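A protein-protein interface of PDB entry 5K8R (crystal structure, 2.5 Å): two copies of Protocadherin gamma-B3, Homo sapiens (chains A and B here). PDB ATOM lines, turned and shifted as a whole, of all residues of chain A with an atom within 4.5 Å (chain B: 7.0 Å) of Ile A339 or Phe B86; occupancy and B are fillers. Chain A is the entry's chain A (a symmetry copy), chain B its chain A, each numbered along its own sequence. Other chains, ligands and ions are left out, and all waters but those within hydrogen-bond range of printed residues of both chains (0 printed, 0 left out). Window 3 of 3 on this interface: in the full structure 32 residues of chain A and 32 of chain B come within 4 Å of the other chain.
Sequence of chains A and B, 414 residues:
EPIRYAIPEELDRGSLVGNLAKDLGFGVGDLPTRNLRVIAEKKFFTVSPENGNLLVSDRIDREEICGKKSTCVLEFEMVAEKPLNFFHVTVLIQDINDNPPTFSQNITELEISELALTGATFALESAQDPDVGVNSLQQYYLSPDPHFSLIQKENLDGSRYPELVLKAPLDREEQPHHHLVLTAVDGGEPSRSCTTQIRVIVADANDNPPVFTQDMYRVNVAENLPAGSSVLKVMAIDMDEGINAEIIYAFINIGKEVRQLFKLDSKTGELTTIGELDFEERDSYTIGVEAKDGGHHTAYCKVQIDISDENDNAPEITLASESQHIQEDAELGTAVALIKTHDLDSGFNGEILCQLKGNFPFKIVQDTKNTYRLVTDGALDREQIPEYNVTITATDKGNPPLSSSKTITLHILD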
ATOM      1  N   ILE A 317      -8.658   8.504 -28.396  1.00  0.00           N
ATOM      2  CA  ILE A 317      -8.486   9.407 -27.264  1.00  0.00           C
ATOM      3  C   ILE A 317      -8.623   8.604 -25.980  1.00  0.00           C
ATOM      4  O   ILE A 317      -9.559   7.808 -25.833  1.00  0.00           O
ATOM      5  CB  ILE A 317      -9.511  10.554 -27.298  1.00  0.00           C
ATOM      6  CG1 ILE A 317      -9.483  11.261 -28.653  1.00  0.00           C
ATOM      7  CG2 ILE A 317      -9.241  11.543 -26.174  1.00  0.00           C
ATOM      8  CD1 ILE A 317     -10.562  12.310 -28.809  1.00  0.00           C
ATOM      9  N   THR A 318      -7.695   8.812 -25.052  1.00  0.00           N
ATOM     10  CA  THR A 318      -7.750   8.222 -23.724  1.00  0.00           C
ATOM     11  C   THR A 318      -7.722   9.343 -22.694  1.00  0.00           C
ATOM     12  O   THR A 318      -6.937  10.287 -22.817  1.00  0.00           O
ATOM     13  CB  THR A 318      -6.586   7.256 -23.490  1.00  0.00           C
ATOM     14  OG1 THR A 318      -6.529   6.307 -24.561  1.00  0.00           O
ATOM     15  CG2 THR A 318      -6.768   6.514 -22.177  1.00  0.00           C
ATOM     16  N   LEU A 319      -8.581   9.243 -21.685  1.00  0.00           N
ATOM     17  CA  LEU A 319      -8.772  10.321 -20.728  1.00  0.00           C
ATOM     18  C   LEU A 319      -8.495   9.846 -19.309  1.00  0.00           C
ATOM     19  O   LEU A 319      -8.700   8.675 -18.974  1.00  0.00           O
ATOM     20  CB  LEU A 319     -10.193  10.889 -20.818  1.00  0.00           C
ATOM     21  CG  LEU A 319     -10.583  11.475 -22.176  1.00  0.00           C
ATOM     22  CD1 LEU A 319     -12.011  11.995 -22.151  1.00  0.00           C
ATOM     23  CD2 LEU A 319      -9.614  12.576 -22.579  1.00  0.00           C
ATOM     24  N   ALA A 337      -7.799  17.224 -16.409  1.00  0.00           N
ATOM     25  CA  ALA A 337      -7.909  15.970 -17.136  1.00  0.00           C
ATOM     26  C   ALA A 337      -6.645  15.750 -17.953  1.00  0.00           C
ATOM     27  O   ALA A 337      -5.958  16.702 -18.334  1.00  0.00           O
ATOM     28  CB  ALA A 337      -9.143  15.950 -18.046  1.00  0.00           C
ATOM     29  N   LEU A 338      -6.345  14.480 -18.212  1.00  0.00           N
ATOM     30  CA  LEU A 338      -5.204  14.077 -19.020  1.00  0.00           C
ATOM     31  C   LEU A 338      -5.706  13.444 -20.309  1.00  0.00           C
ATOM     32  O   LEU A 338      -6.609  12.598 -20.280  1.00  0.00           O
ATOM     33  CB  LEU A 338      -4.310  13.096 -18.257  1.00  0.00           C
ATOM     34  CG  LEU A 338      -3.717  13.591 -16.937  1.00  0.00           C
ATOM     35  CD1 LEU A 338      -2.831  12.524 -16.310  1.00  0.00           C
ATOM     36  CD2 LEU A 338      -2.940  14.881 -17.146  1.00  0.00           C
ATOM     37  N   ILE A 339      -5.122  13.856 -21.432  1.00  0.00           N
ATOM     38  CA  ILE A 339      -5.527  13.409 -22.760  1.00  0.00           C
ATOM     39  C   ILE A 339      -4.350  12.691 -23.404  1.00  0.00           C
ATOM     40  O   ILE A 339      -3.217  13.187 -23.367  1.00  0.00           O
ATOM     41  CB  ILE A 339      -5.995  14.588 -23.633  1.00  0.00           C
ATOM     42  CG1 ILE A 339      -7.054  15.409 -22.893  1.00  0.00           C
ATOM     43  CG2 ILE A 339      -6.535  14.087 -24.963  1.00  0.00           C
ATOM     44  CD1 ILE A 339      -7.487  16.656 -23.630  1.00  0.00           C
ATOM     45  N   LYS A 340      -4.620  11.528 -23.999  1.00  0.00           N
ATOM     46  CA  LYS A 340      -3.591  10.693 -24.622  1.00  0.00           C
ATOM     47  C   LYS A 340      -4.155  10.167 -25.939  1.00  0.00           C
ATOM     48  O   LYS A 340      -4.971   9.241 -25.945  1.00  0.00           O
ATOM     49  CB  LYS A 340      -3.175   9.555 -23.698  1.00  0.00           C
ATOM     50  CG  LYS A 340      -2.279   8.500 -24.336  1.00  0.00           C
ATOM     51  CD  LYS A 340      -0.964   9.088 -24.821  1.00  0.00           C
ATOM     52  CE  LYS A 340       0.071   7.996 -25.062  1.00  0.00           C
ATOM     53  NZ  LYS A 340      -0.445   6.911 -25.939  1.00  0.00           N
ATOM     54  N   THR A 341      -3.720  10.759 -27.046  1.00  0.00           N
ATOM     55  CA  THR A 341      -4.161  10.361 -28.374  1.00  0.00           C
ATOM     56  C   THR A 341      -3.168   9.379 -28.984  1.00  0.00           C
ATOM     57  O   THR A 341      -1.972   9.417 -28.688  1.00  0.00           O
ATOM     58  CB  THR A 341      -4.307  11.576 -29.294  1.00  0.00           C
ATOM     59  OG1 THR A 341      -3.011  12.111 -29.592  1.00  0.00           O
ATOM     60  CG2 THR A 341      -5.149  12.653 -28.627  1.00  0.00           C
ATOM     61  N   CYS A 354      -5.577  17.453 -31.849  1.00  0.00           N
ATOM     62  CA  CYS A 354      -6.526  17.309 -30.754  1.00  0.00           C
ATOM     63  C   CYS A 354      -7.033  18.684 -30.345  1.00  0.00           C
ATOM     64  O   CYS A 354      -6.235  19.588 -30.073  1.00  0.00           O
ATOM     65  CB  CYS A 354      -5.879  16.602 -29.562  1.00  0.00           C
ATOM     66  SG  CYS A 354      -6.926  16.493 -28.099  1.00  0.00           S
ATOM     67  N   ILE A 364      -6.994  23.273 -23.617  1.00  0.00           N
ATOM     68  CA  ILE A 364      -6.065  22.168 -23.830  1.00  0.00           C
ATOM     69  C   ILE A 364      -4.652  22.719 -23.969  1.00  0.00           C
ATOM     70  O   ILE A 364      -4.394  23.612 -24.787  1.00  0.00           O
ATOM     71  CB  ILE A 364      -6.468  21.348 -25.067  1.00  0.00           C
ATOM     72  CG1 ILE A 364      -7.727  20.531 -24.775  1.00  0.00           C
ATOM     73  CG2 ILE A 364      -5.328  20.434 -25.498  1.00  0.00           C
ATOM     74  CD1 ILE A 364      -8.138  19.616 -25.908  1.00  0.00           C
ATOM     75  N   ASN A 370       1.645  13.469 -28.233  1.00  0.00           N
ATOM     76  CA  ASN A 370       0.397  12.733 -28.070  1.00  0.00           C
ATOM     77  C   ASN A 370      -0.183  12.856 -26.663  1.00  0.00           C
ATOM     78  O   ASN A 370      -1.067  12.074 -26.299  1.00  0.00           O
ATOM     79  CB  ASN A 370       0.598  11.258 -28.423  1.00  0.00           C
ATOM     80  CG  ASN A 370       0.921  11.049 -29.888  1.00  0.00           C
ATOM     81  OD1 ASN A 370       0.436  11.779 -30.753  1.00  0.00           O
ATOM     82  ND2 ASN A 370       1.746  10.049 -30.176  1.00  0.00           N
ATOM     83  N   THR A 371       0.283  13.814 -25.865  1.00  0.00           N
ATOM     84  CA  THR A 371      -0.234  14.012 -24.516  1.00  0.00           C
ATOM     85  C   THR A 371      -0.631  15.468 -24.328  1.00  0.00           C
ATOM     86  O   THR A 371       0.136  16.377 -24.663  1.00  0.00           O
ATOM     87  CB  THR A 371       0.792  13.608 -23.450  1.00  0.00           C
ATOM     88  OG1 THR A 371       1.986  14.382 -23.611  1.00  0.00           O
ATOM     89  CG2 THR A 371       1.127  12.127 -23.563  1.00  0.00           C
ATOM     90  N   TYR A 372      -1.829  15.681 -23.787  1.00  0.00           N
ATOM     91  CA  TYR A 372      -2.366  17.009 -23.538  1.00  0.00           C
ATOM     92  C   TYR A 372      -2.906  17.069 -22.116  1.00  0.00           C
ATOM     93  O   TYR A 372      -3.104  16.042 -21.461  1.00  0.00           O
ATOM     94  CB  TYR A 372      -3.480  17.367 -24.537  1.00  0.00           C
ATOM     95  CG  TYR A 372      -3.099  17.190 -25.993  1.00  0.00           C
ATOM     96  CD1 TYR A 372      -2.702  18.274 -26.764  1.00  0.00           C
ATOM     97  CD2 TYR A 372      -3.145  15.938 -26.596  1.00  0.00           C
ATOM     98  CE1 TYR A 372      -2.356  18.116 -28.094  1.00  0.00           C
ATOM     99  CE2 TYR A 372      -2.797  15.771 -27.923  1.00  0.00           C
ATOM    100  CZ  TYR A 372      -2.404  16.862 -28.668  1.00  0.00           C
ATOM    101  OH  TYR A 372      -2.061  16.700 -29.991  1.00  0.00           O
ATOM    102  N   ILE A 392     -13.844  16.179 -26.165  1.00  0.00           N
ATOM    103  CA  ILE A 392     -12.535  16.287 -26.798  1.00  0.00           C
ATOM    104  C   ILE A 392     -12.602  15.594 -28.150  1.00  0.00           C
ATOM    105  O   ILE A 392     -13.124  14.477 -28.259  1.00  0.00           O
ATOM    106  CB  ILE A 392     -11.438  15.668 -25.915  1.00  0.00           C
ATOM    107  CG1 ILE A 392     -11.434  16.320 -24.531  1.00  0.00           C
ATOM    108  CG2 ILE A 392     -10.079  15.813 -26.576  1.00  0.00           C
ATOM    109  CD1 ILE A 392     -11.142  17.804 -24.554  1.00  0.00           C
ATOM    110  N   GLU B   1      11.132   9.372 -16.584  1.00  0.00           N
ATOM    111  CA  GLU B   1      10.827  10.638 -17.238  1.00  0.00           C
ATOM    112  C   GLU B   1      11.653  10.816 -18.527  1.00  0.00           C
ATOM    113  O   GLU B   1      12.285  11.860 -18.695  1.00  0.00           O
ATOM    114  CB  GLU B   1      11.070  11.809 -16.281  1.00  0.00           C
ATOM    115  CG  GLU B   1       9.968  12.009 -15.254  1.00  0.00           C
ATOM    116  CD  GLU B   1      10.367  11.535 -13.870  1.00  0.00           C
ATOM    117  OE1 GLU B   1      11.552  11.191 -13.678  1.00  0.00           O
ATOM    118  OE2 GLU B   1       9.496  11.506 -12.975  1.00  0.00           O
ATOM    119  N   ILE B  39      -2.252   2.838 -17.618  1.00  0.00           N
ATOM    120  CA  ILE B  39      -3.269   3.097 -18.629  1.00  0.00           C
ATOM    121  C   ILE B  39      -2.897   2.468 -19.968  1.00  0.00           C
ATOM    122  O   ILE B  39      -2.007   2.950 -20.669  1.00  0.00           O
ATOM    123  CB  ILE B  39      -3.495   4.607 -18.828  1.00  0.00           C
ATOM    124  CG1 ILE B  39      -4.010   5.244 -17.535  1.00  0.00           C
ATOM    125  CG2 ILE B  39      -4.466   4.854 -19.972  1.00  0.00           C
ATOM    126  CD1 ILE B  39      -5.415   4.824 -17.166  1.00  0.00           C
ATOM    127  N   GLU B  77       1.341   4.518 -20.369  1.00  0.00           N
ATOM    128  CA  GLU B  77       1.386   5.729 -19.561  1.00  0.00           C
ATOM    129  C   GLU B  77       0.884   5.412 -18.160  1.00  0.00           C
ATOM    130  O   GLU B  77      -0.231   4.900 -17.998  1.00  0.00           O
ATOM    131  CB  GLU B  77       0.541   6.839 -20.191  1.00  0.00           C
ATOM    132  CG  GLU B  77       0.960   7.233 -21.599  1.00  0.00           C
ATOM    133  CD  GLU B  77       2.130   8.198 -21.616  1.00  0.00           C
ATOM    134  OE1 GLU B  77       2.518   8.685 -20.534  1.00  0.00           O
ATOM    135  OE2 GLU B  77       2.658   8.473 -22.714  1.00  0.00           O
ATOM    136  N   MET B  78       1.704   5.708 -17.156  1.00  0.00           N
ATOM    137  CA  MET B  78       1.271   5.661 -15.766  1.00  0.00           C
ATOM    138  C   MET B  78       0.829   7.059 -15.355  1.00  0.00           C
ATOM    139  O   MET B  78       1.625   8.004 -15.404  1.00  0.00           O
ATOM    140  CB  MET B  78       2.388   5.167 -14.847  1.00  0.00           C
ATOM    141  CG  MET B  78       1.952   5.031 -13.393  1.00  0.00           C
ATOM    142  SD  MET B  78       3.305   5.122 -12.203  1.00  0.00           S
ATOM    143  CE  MET B  78       3.705   6.864 -12.279  1.00  0.00           C
ATOM    144  N   VAL B  79      -0.435   7.185 -14.966  1.00  0.00           N
ATOM    145  CA  VAL B  79      -0.988   8.473 -14.572  1.00  0.00           C
ATOM    146  C   VAL B  79      -1.113   8.659 -13.063  1.00  0.00           C
ATOM    147  O   VAL B  79      -1.553   7.764 -12.342  1.00  0.00           O
ATOM    148  CB  VAL B  79      -2.370   8.709 -15.215  1.00  0.00           C
ATOM    149  CG1 VAL B  79      -3.365   7.668 -14.729  1.00  0.00           C
ATOM    150  CG2 VAL B  79      -2.863  10.115 -14.907  1.00  0.00           C
ATOM    151  N   ALA B  80      -0.719   9.842 -12.608  1.00  0.00           N
ATOM    152  CA  ALA B  80      -0.780  10.216 -11.207  1.00  0.00           C
ATOM    153  C   ALA B  80      -1.710  11.410 -11.069  1.00  0.00           C
ATOM    154  O   ALA B  80      -1.922  12.167 -12.020  1.00  0.00           O
ATOM    155  CB  ALA B  80       0.605  10.564 -10.649  1.00  0.00           C
ATOM    156  N   PRO B  83      -0.731  16.478  -8.198  1.00  0.00           N
ATOM    157  CA  PRO B  83      -1.437  16.935  -9.400  1.00  0.00           C
ATOM    158  C   PRO B  83      -1.478  15.866 -10.493  1.00  0.00           C
ATOM    159  O   PRO B  83      -0.716  14.901 -10.433  1.00  0.00           O
ATOM    160  CB  PRO B  83      -0.610  18.138  -9.846  1.00  0.00           C
ATOM    161  CG  PRO B  83       0.774  17.781  -9.441  1.00  0.00           C
ATOM    162  CD  PRO B  83       0.654  16.984  -8.161  1.00  0.00           C
ATOM    163  N   LEU B  84      -2.363  16.038 -11.472  1.00  0.00           N
ATOM    164  CA  LEU B  84      -2.462  15.086 -12.572  1.00  0.00           C
ATOM    165  C   LEU B  84      -1.243  15.193 -13.479  1.00  0.00           C
ATOM    166  O   LEU B  84      -0.832  16.295 -13.857  1.00  0.00           O
ATOM    167  CB  LEU B  84      -3.738  15.332 -13.375  1.00  0.00           C
ATOM    168  CG  LEU B  84      -5.030  14.722 -12.831  1.00  0.00           C
ATOM    169  CD1 LEU B  84      -6.223  15.235 -13.613  1.00  0.00           C
ATOM    170  CD2 LEU B  84      -4.964  13.205 -12.896  1.00  0.00           C
ATOM    171  N   ASN B  85      -0.668  14.044 -13.831  1.00  0.00           N
ATOM    172  CA  ASN B  85       0.518  14.007 -14.673  1.00  0.00           C
ATOM    173  C   ASN B  85       0.634  12.637 -15.329  1.00  0.00           C
ATOM    174  O   ASN B  85       0.294  11.616 -14.722  1.00  0.00           O
ATOM    175  CB  ASN B  85       1.789  14.311 -13.870  1.00  0.00           C
ATOM    176  CG  ASN B  85       2.128  15.790 -13.852  1.00  0.00           C
ATOM    177  OD1 ASN B  85       1.925  16.498 -14.839  1.00  0.00           O
ATOM    178  ND2 ASN B  85       2.649  16.264 -12.725  1.00  0.00           N
ATOM    179  N   PHE B  86       1.185  12.631 -16.540  1.00  0.00           N
ATOM    180  CA  PHE B  86       1.434  11.410 -17.292  1.00  0.00           C
ATOM    181  C   PHE B  86       2.917  11.053 -17.145  1.00  0.00           C
ATOM    182  O   PHE B  86       3.774  11.936 -17.090  1.00  0.00           O
ATOM    183  CB  PHE B  86       1.077  11.600 -18.766  1.00  0.00           C
ATOM    184  CG  PHE B  86      -0.332  11.205 -19.103  1.00  0.00           C
ATOM    185  CD1 PHE B  86      -0.993  10.242 -18.359  1.00  0.00           C
ATOM    186  CD2 PHE B  86      -0.996  11.795 -20.165  1.00  0.00           C
ATOM    187  CE1 PHE B  86      -2.290   9.876 -18.666  1.00  0.00           C
ATOM    188  CE2 PHE B  86      -2.292  11.435 -20.479  1.00  0.00           C
ATOM    189  CZ  PHE B  86      -2.941  10.473 -19.728  1.00  0.00           C
ATOM    190  N   PHE B  87       3.208   9.759 -17.077  1.00  0.00           N
ATOM    191  CA  PHE B  87       4.569   9.252 -16.917  1.00  0.00           C
ATOM    192  C   PHE B  87       4.756   8.114 -17.909  1.00  0.00           C
ATOM    193  O   PHE B  87       4.235   7.014 -17.699  1.00  0.00           O
ATOM    194  CB  PHE B  87       4.830   8.787 -15.486  1.00  0.00           C
ATOM    195  CG  PHE B  87       4.746   9.888 -14.468  1.00  0.00           C
ATOM    196  CD1 PHE B  87       5.838  10.704 -14.222  1.00  0.00           C
ATOM    197  CD2 PHE B  87       3.578  10.107 -13.758  1.00  0.00           C
ATOM    198  CE1 PHE B  87       5.765  11.718 -13.286  1.00  0.00           C
ATOM    199  CE2 PHE B  87       3.499  11.119 -12.819  1.00  0.00           C
ATOM    200  CZ  PHE B  87       4.595  11.926 -12.584  1.00  0.00           C
ATOM    201  N   HIS B  88       5.492   8.378 -18.985  1.00  0.00           N
ATOM    202  CA  HIS B  88       5.655   7.391 -20.043  1.00  0.00           C
ATOM    203  C   HIS B  88       6.602   6.287 -19.592  1.00  0.00           C
ATOM    204  O   HIS B  88       7.711   6.558 -19.122  1.00  0.00           O
ATOM    205  CB  HIS B  88       6.180   8.055 -21.315  1.00  0.00           C
ATOM    206  CG  HIS B  88       6.168   7.156 -22.512  1.00  0.00           C
ATOM    207  ND1 HIS B  88       5.010   6.818 -23.178  1.00  0.00           N
ATOM    208  CD2 HIS B  88       7.173   6.519 -23.160  1.00  0.00           C
ATOM    209  CE1 HIS B  88       5.300   6.014 -24.185  1.00  0.00           C
ATOM    210  NE2 HIS B  88       6.607   5.817 -24.196  1.00  0.00           N
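The backbone carbonyl oxygen (O) of Glu B77 sits at hydrogen-bond distance from the backbone NH (N) of Ile B39 (2.9 Å).
The side-chain carboxylate (OE2) of Glu B77 sits at hydrogen-bond distance from a ring nitrogen (ND1) of His B88, 2.9 Å away.
The backbone NH (N) of Asn B85 is in hydrogen-bond range of the backbone carbonyl oxygen (O) of Ala B80, 2.9 Å away.
O of Thr A318 sits at hydrogen-bond distance from N of Lys A340, at 2.9 Å.
The backbone carbonyl oxygen (O) of Ile A339 is in hydrogen-bond range of the backbone NH (N) of Tyr A372, 2.9 Å away.
Among the printed residues, merely in contact across the chains: Leu A338 with Val B79, Leu A338 with Phe B86, Ile A339 with Phe B86, Lys A340 with Glu B77, Thr A318 with Ile B39, Leu A338 with Asn B85, Ala A337 with Leu B84, Lys A340 with Phe B86 and Leu A338 with Leu B84.
Of the printed residues of chain B, Thr A318 touches Ile B39 (3.6 Å).
Ile A339 touches just one residue of chain B: Phe B86.
Of the printed residues of chain A, Ile B39 touches Thr A318.
Ala B80 touches none of the printed residues of chain A.
Phe B86 touches three residues of chain A.
The nearest residue of chain A that does not touch Phe B86 is Thr A371 (4.02 Å).
The nearest printed residue of chain A that does not touch Ile B39 is Leu A319 (5.4 Å).
Of the 12 printed residues of chain B, 6 touch a printed residue of chain A.
Hydrophobic or aromatic side chains of chain B that line the printed part of chain A: Ile B39, Val B79, Leu B84 and Phe B86.
Along chain B the printed residues that touch a printed residue of chain A span positions 39 to 86.
Among the printed residues, 9 pairs touch across the chains.
Among the printed residues, no Asp or Glu carboxylate lies within 4 Å of a Lys or Arg side-chain nitrogen of the other chain.
No position is printed for both chains.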
